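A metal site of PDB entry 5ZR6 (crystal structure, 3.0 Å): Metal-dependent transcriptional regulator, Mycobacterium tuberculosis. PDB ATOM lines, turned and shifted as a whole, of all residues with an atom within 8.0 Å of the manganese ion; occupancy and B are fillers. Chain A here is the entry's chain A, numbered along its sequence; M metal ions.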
ATOM      1  N   VAL A   3       3.741   5.477  -2.094  1.00  0.00           N
ATOM      2  CA  VAL A   3       3.995   5.067  -0.719  1.00  0.00           C
ATOM      3  C   VAL A   3       5.403   5.488  -0.300  1.00  0.00           C
ATOM      4  O   VAL A   3       6.396   4.977  -0.815  1.00  0.00           O
ATOM      5  CB  VAL A   3       3.787   3.563  -0.556  1.00  0.00           C
ATOM      6  CG1 VAL A   3       2.311   3.264  -0.339  1.00  0.00           C
ATOM      7  CG2 VAL A   3       4.270   2.823  -1.790  1.00  0.00           C
ATOM      8  N   GLN A   5       7.265   5.065   2.330  1.00  0.00           N
ATOM      9  CA  GLN A   5       8.179   4.085   2.916  1.00  0.00           C
ATOM     10  C   GLN A   5       8.839   3.216   1.865  1.00  0.00           C
ATOM     11  O   GLN A   5       9.967   2.742   2.065  1.00  0.00           O
ATOM     12  CB  GLN A   5       7.430   3.204   3.926  1.00  0.00           C
ATOM     13  CG  GLN A   5       6.584   3.981   4.930  1.00  0.00           C
ATOM     14  CD  GLN A   5       5.707   3.070   5.764  1.00  0.00           C
ATOM     15  OE1 GLN A   5       6.055   2.698   6.884  1.00  0.00           O
ATOM     16  NE2 GLN A   5       4.548   2.698   5.213  1.00  0.00           N
ATOM     17  N   ASP A   6       8.152   2.984   0.737  1.00  0.00           N
ATOM     18  CA  ASP A   6       8.736   2.176  -0.333  1.00  0.00           C
ATOM     19  C   ASP A   6      10.014   2.795  -0.878  1.00  0.00           C
ATOM     20  O   ASP A   6      10.936   2.074  -1.261  1.00  0.00           O
ATOM     21  CB  ASP A   6       7.718   1.978  -1.448  1.00  0.00           C
ATOM     22  CG  ASP A   6       6.999   0.656  -1.366  1.00  0.00           C
ATOM     23  OD1 ASP A   6       7.201  -0.069  -0.365  1.00  0.00           O
ATOM     24  OD2 ASP A   6       6.215   0.333  -2.289  1.00  0.00           O
ATOM     25  N   TYR A   7      10.073   4.122  -0.926  1.00  0.00           N
ATOM     26  CA  TYR A   7      11.230   4.803  -1.503  1.00  0.00           C
ATOM     27  C   TYR A   7      12.489   4.567  -0.679  1.00  0.00           C
ATOM     28  O   TYR A   7      13.535   4.207  -1.231  1.00  0.00           O
ATOM     29  CB  TYR A   7      10.942   6.295  -1.659  1.00  0.00           C
ATOM     30  CG  TYR A   7       9.995   6.602  -2.805  1.00  0.00           C
ATOM     31  CD1 TYR A   7       8.621   6.435  -2.659  1.00  0.00           C
ATOM     32  CD2 TYR A   7      10.476   7.033  -4.030  1.00  0.00           C
ATOM     33  CE1 TYR A   7       7.754   6.700  -3.704  1.00  0.00           C
ATOM     34  CE2 TYR A   7       9.620   7.304  -5.078  1.00  0.00           C
ATOM     35  CZ  TYR A   7       8.261   7.138  -4.906  1.00  0.00           C
ATOM     36  OH  TYR A   7       7.400   7.410  -5.946  1.00  0.00           O
ATOM     37  N   LYS A   9      13.245   2.181   1.426  1.00  0.00           N
ATOM     38  CA  LYS A   9      13.665   0.796   1.326  1.00  0.00           C
ATOM     39  C   LYS A   9      14.297   0.515  -0.038  1.00  0.00           C
ATOM     40  O   LYS A   9      15.293  -0.201  -0.130  1.00  0.00           O
ATOM     41  CB  LYS A   9      12.485  -0.143   1.563  1.00  0.00           C
ATOM     42  CG  LYS A   9      12.884  -1.608   1.667  1.00  0.00           C
ATOM     43  CD  LYS A   9      11.710  -2.555   1.510  1.00  0.00           C
ATOM     44  CE  LYS A   9      11.017  -2.351   0.171  1.00  0.00           C
ATOM     45  NZ  LYS A   9       9.874  -3.300   0.001  1.00  0.00           N
ATOM     46  N   VAL A  10      13.727   1.089  -1.095  1.00  0.00           N
ATOM     47  CA  VAL A  10      14.254   0.851  -2.436  1.00  0.00           C
ATOM     48  C   VAL A  10      15.611   1.521  -2.609  1.00  0.00           C
ATOM     49  O   VAL A  10      16.536   0.925  -3.176  1.00  0.00           O
ATOM     50  CB  VAL A  10      13.242   1.315  -3.495  1.00  0.00           C
ATOM     51  CG1 VAL A  10      13.931   1.501  -4.831  1.00  0.00           C
ATOM     52  CG2 VAL A  10      12.104   0.311  -3.628  1.00  0.00           C
ATOM     53  N   ILE A  31       9.797   0.944  -8.287  1.00  0.00           N
ATOM     54  CA  ILE A  31       8.713   1.101  -7.332  1.00  0.00           C
ATOM     55  C   ILE A  31       7.375   0.833  -7.999  1.00  0.00           C
ATOM     56  O   ILE A  31       6.426   0.348  -7.366  1.00  0.00           O
ATOM     57  CB  ILE A  31       8.782   2.508  -6.685  1.00  0.00           C
ATOM     58  CG1 ILE A  31       9.960   2.575  -5.710  1.00  0.00           C
ATOM     59  CG2 ILE A  31       7.476   2.863  -5.988  1.00  0.00           C
ATOM     60  CD1 ILE A  31       9.851   3.672  -4.693  1.00  0.00           C
ATOM     61  N   MET A  72      12.437  -0.585   7.444  1.00  0.00           N
ATOM     62  CA  MET A  72      11.594  -1.159   6.403  1.00  0.00           C
ATOM     63  C   MET A  72      12.183  -2.450   5.855  1.00  0.00           C
ATOM     64  O   MET A  72      11.463  -3.427   5.632  1.00  0.00           O
ATOM     65  CB  MET A  72      11.405  -0.144   5.261  1.00  0.00           C
ATOM     66  CG  MET A  72      10.316   0.891   5.517  1.00  0.00           C
ATOM     67  SD  MET A  72       8.670   0.198   5.719  1.00  0.00           S
ATOM     68  CE  MET A  72       8.397   0.477   7.467  1.00  0.00           C
ATOM     69  N   HIS A  76      10.311  -6.182   5.897  1.00  0.00           N
ATOM     70  CA  HIS A  76      10.146  -6.906   4.640  1.00  0.00           C
ATOM     71  C   HIS A  76      10.818  -8.276   4.693  1.00  0.00           C
ATOM     72  O   HIS A  76      10.239  -9.279   4.277  1.00  0.00           O
ATOM     73  CB  HIS A  76      10.722  -6.080   3.483  1.00  0.00           C
ATOM     74  CG  HIS A  76      10.699  -6.794   2.162  1.00  0.00           C
ATOM     75  ND1 HIS A  76       9.663  -6.667   1.265  1.00  0.00           N
ATOM     76  CD2 HIS A  76      11.588  -7.629   1.590  1.00  0.00           C
ATOM     77  CE1 HIS A  76       9.914  -7.392   0.200  1.00  0.00           C
ATOM     78  NE2 HIS A  76      11.079  -7.991   0.366  1.00  0.00           N
ATOM     79  N   HIS A  95       7.957 -12.334  -2.055  1.00  0.00           N
ATOM     80  CA  HIS A  95       8.326 -10.922  -2.187  1.00  0.00           C
ATOM     81  C   HIS A  95       7.107 -10.048  -2.428  1.00  0.00           C
ATOM     82  O   HIS A  95       6.999  -8.953  -1.851  1.00  0.00           O
ATOM     83  CB  HIS A  95       9.345 -10.744  -3.299  1.00  0.00           C
ATOM     84  CG  HIS A  95       9.919  -9.362  -3.354  1.00  0.00           C
ATOM     85  ND1 HIS A  95      10.939  -8.946  -2.528  1.00  0.00           N
ATOM     86  CD2 HIS A  95       9.600  -8.285  -4.122  1.00  0.00           C
ATOM     87  CE1 HIS A  95      11.233  -7.679  -2.791  1.00  0.00           C
ATOM     88  NE2 HIS A  95      10.427  -7.264  -3.743  1.00  0.00           N
ATOM     89  N   ASP A  96       6.188 -10.486  -3.284  1.00  0.00           N
ATOM     90  CA  ASP A  96       4.996  -9.684  -3.534  1.00  0.00           C
ATOM     91  C   ASP A  96       4.105  -9.587  -2.297  1.00  0.00           C
ATOM     92  O   ASP A  96       3.412  -8.578  -2.105  1.00  0.00           O
ATOM     93  CB  ASP A  96       4.208 -10.261  -4.713  1.00  0.00           C
ATOM     94  CG  ASP A  96       5.051 -10.329  -5.982  1.00  0.00           C
ATOM     95  OD1 ASP A  96       5.986  -9.526  -6.113  1.00  0.00           O
ATOM     96  OD2 ASP A  96       4.749 -11.187  -6.838  1.00  0.00           O
ATOM     97  N   GLU A  97       4.138 -10.614  -1.439  1.00  0.00           N
ATOM     98  CA  GLU A  97       3.323 -10.579  -0.223  1.00  0.00           C
ATOM     99  C   GLU A  97       3.915  -9.616   0.798  1.00  0.00           C
ATOM    100  O   GLU A  97       3.225  -8.705   1.284  1.00  0.00           O
ATOM    101  CB  GLU A  97       3.214 -11.981   0.363  1.00  0.00           C
ATOM    102  CG  GLU A  97       2.224 -12.089   1.508  1.00  0.00           C
ATOM    103  CD  GLU A  97       0.792 -12.086   1.037  1.00  0.00           C
ATOM    104  OE1 GLU A  97       0.038 -11.162   1.425  1.00  0.00           O
ATOM    105  OE2 GLU A  97       0.407 -13.005   0.274  1.00  0.00           O
ATOM    106  N   ALA A  98       5.193  -9.793   1.152  1.00  0.00           N
ATOM    107  CA  ALA A  98       5.827  -8.920   2.124  1.00  0.00           C
ATOM    108  C   ALA A  98       5.986  -7.495   1.620  1.00  0.00           C
ATOM    109  O   ALA A  98       6.199  -6.586   2.419  1.00  0.00           O
ATOM    110  CB  ALA A  98       7.197  -9.484   2.519  1.00  0.00           C
ATOM    111  N   GLU A  99       5.867  -7.275   0.303  1.00  0.00           N
ATOM    112  CA  GLU A  99       5.908  -5.915  -0.217  1.00  0.00           C
ATOM    113  C   GLU A  99       4.663  -5.125   0.181  1.00  0.00           C
ATOM    114  O   GLU A  99       4.706  -3.902   0.277  1.00  0.00           O
ATOM    115  CB  GLU A  99       6.059  -5.948  -1.738  1.00  0.00           C
ATOM    116  CG  GLU A  99       6.198  -4.580  -2.401  1.00  0.00           C
ATOM    117  CD  GLU A  99       7.493  -3.886  -2.043  1.00  0.00           C
ATOM    118  OE1 GLU A  99       8.553  -4.545  -2.058  1.00  0.00           O
ATOM    119  OE2 GLU A  99       7.456  -2.676  -1.749  1.00  0.00           O
ATOM    120  N   VAL A 100       3.552  -5.826   0.427  1.00  0.00           N
ATOM    121  CA  VAL A 100       2.317  -5.190   0.876  1.00  0.00           C
ATOM    122  C   VAL A 100       2.174  -5.243   2.386  1.00  0.00           C
ATOM    123  O   VAL A 100       1.699  -4.288   3.003  1.00  0.00           O
ATOM    124  CB  VAL A 100       1.102  -5.837   0.171  1.00  0.00           C
ATOM    125  CG1 VAL A 100      -0.161  -5.052   0.461  1.00  0.00           C
ATOM    126  CG2 VAL A 100       1.351  -5.939  -1.323  1.00  0.00           C
ATOM    127  N   LEU A 101       2.572  -6.362   3.000  1.00  0.00           N
ATOM    128  CA  LEU A 101       2.464  -6.534   4.446  1.00  0.00           C
ATOM    129  C   LEU A 101       3.411  -5.640   5.224  1.00  0.00           C
ATOM    130  O   LEU A 101       3.251  -5.516   6.446  1.00  0.00           O
ATOM    131  CB  LEU A 101       2.719  -7.997   4.811  1.00  0.00           C
ATOM    132  CG  LEU A 101       1.526  -8.824   5.278  1.00  0.00           C
ATOM    133  CD1 LEU A 101       2.000 -10.085   5.975  1.00  0.00           C
ATOM    134  CD2 LEU A 101       0.650  -7.992   6.210  1.00  0.00           C
ATOM    135  N   GLU A 102       4.387  -5.009   4.573  1.00  0.00           N
ATOM    136  CA  GLU A 102       5.409  -4.251   5.285  1.00  0.00           C
ATOM    137  C   GLU A 102       4.879  -2.953   5.884  1.00  0.00           C
ATOM    138  O   GLU A 102       5.470  -2.455   6.846  1.00  0.00           O
ATOM    139  CB  GLU A 102       6.574  -3.952   4.341  1.00  0.00           C
ATOM    140  CG  GLU A 102       6.179  -3.201   3.087  1.00  0.00           C
ATOM    141  CD  GLU A 102       7.276  -3.150   2.056  1.00  0.00           C
ATOM    142  OE1 GLU A 102       7.127  -2.422   1.047  1.00  0.00           O
ATOM    143  OE2 GLU A 102       8.295  -3.861   2.225  1.00  0.00           O
ATOM    144  N   HIS A 103       3.791  -2.393   5.350  1.00  0.00           N
ATOM    145  CA  HIS A 103       3.267  -1.123   5.824  1.00  0.00           C
ATOM    146  C   HIS A 103       2.124  -1.266   6.811  1.00  0.00           C
ATOM    147  O   HIS A 103       1.531  -0.245   7.198  1.00  0.00           O
ATOM    148  CB  HIS A 103       2.819  -0.245   4.643  1.00  0.00           C
ATOM    149  CG  HIS A 103       3.664  -0.388   3.425  1.00  0.00           C
ATOM    150  ND1 HIS A 103       4.808   0.363   3.216  1.00  0.00           N
ATOM    151  CD2 HIS A 103       3.515  -1.162   2.320  1.00  0.00           C
ATOM    152  CE1 HIS A 103       5.335   0.043   2.057  1.00  0.00           C
ATOM    153  NE2 HIS A 103       4.579  -0.879   1.490  1.00  0.00           N
HETATM  154 MN    MN M   1       5.704  -2.074  -0.254  1.00  0.00          MN
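The side-chain carboxylate (OE2) of Glu 102 lies within salt-bridge range of the side-chain amino group (NZ) of Lys 9, at 2.8 Å.
The side-chain carboxylate (OE2) of Glu 102 lies within hydrogen-bond range of a ring nitrogen (ND1) of His 76, 3.3 Å away.
NZ of Lys 9 is in salt-bridge range of OE1 of Glu 99, at 2.7 Å.
The side-chain amide nitrogen (NE2) of Gln 5 is in hydrogen-bond range of a ring nitrogen (ND1) of His 103 (3.1 Å).
Of the 18 residues printed, 4 come within 4 Å of the manganese ion.
The nearest printed residue that does not touch the manganese ion is Lys 9 (4.4 Å).
The manganese ion is bound by the side-chain carboxylate (OE1) of Glu 102.
The manganese ion is bound by O of Glu 99 (2.1 Å).
The manganese ion is bound by the side-chain carboxylate (OE2) of Glu 99, 2.4 Å away.
NE2 of His 103 binds the manganese ion, 2.4 Å away.
OD1 of Asp 6 binds the manganese ion, at 2.5 Å.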
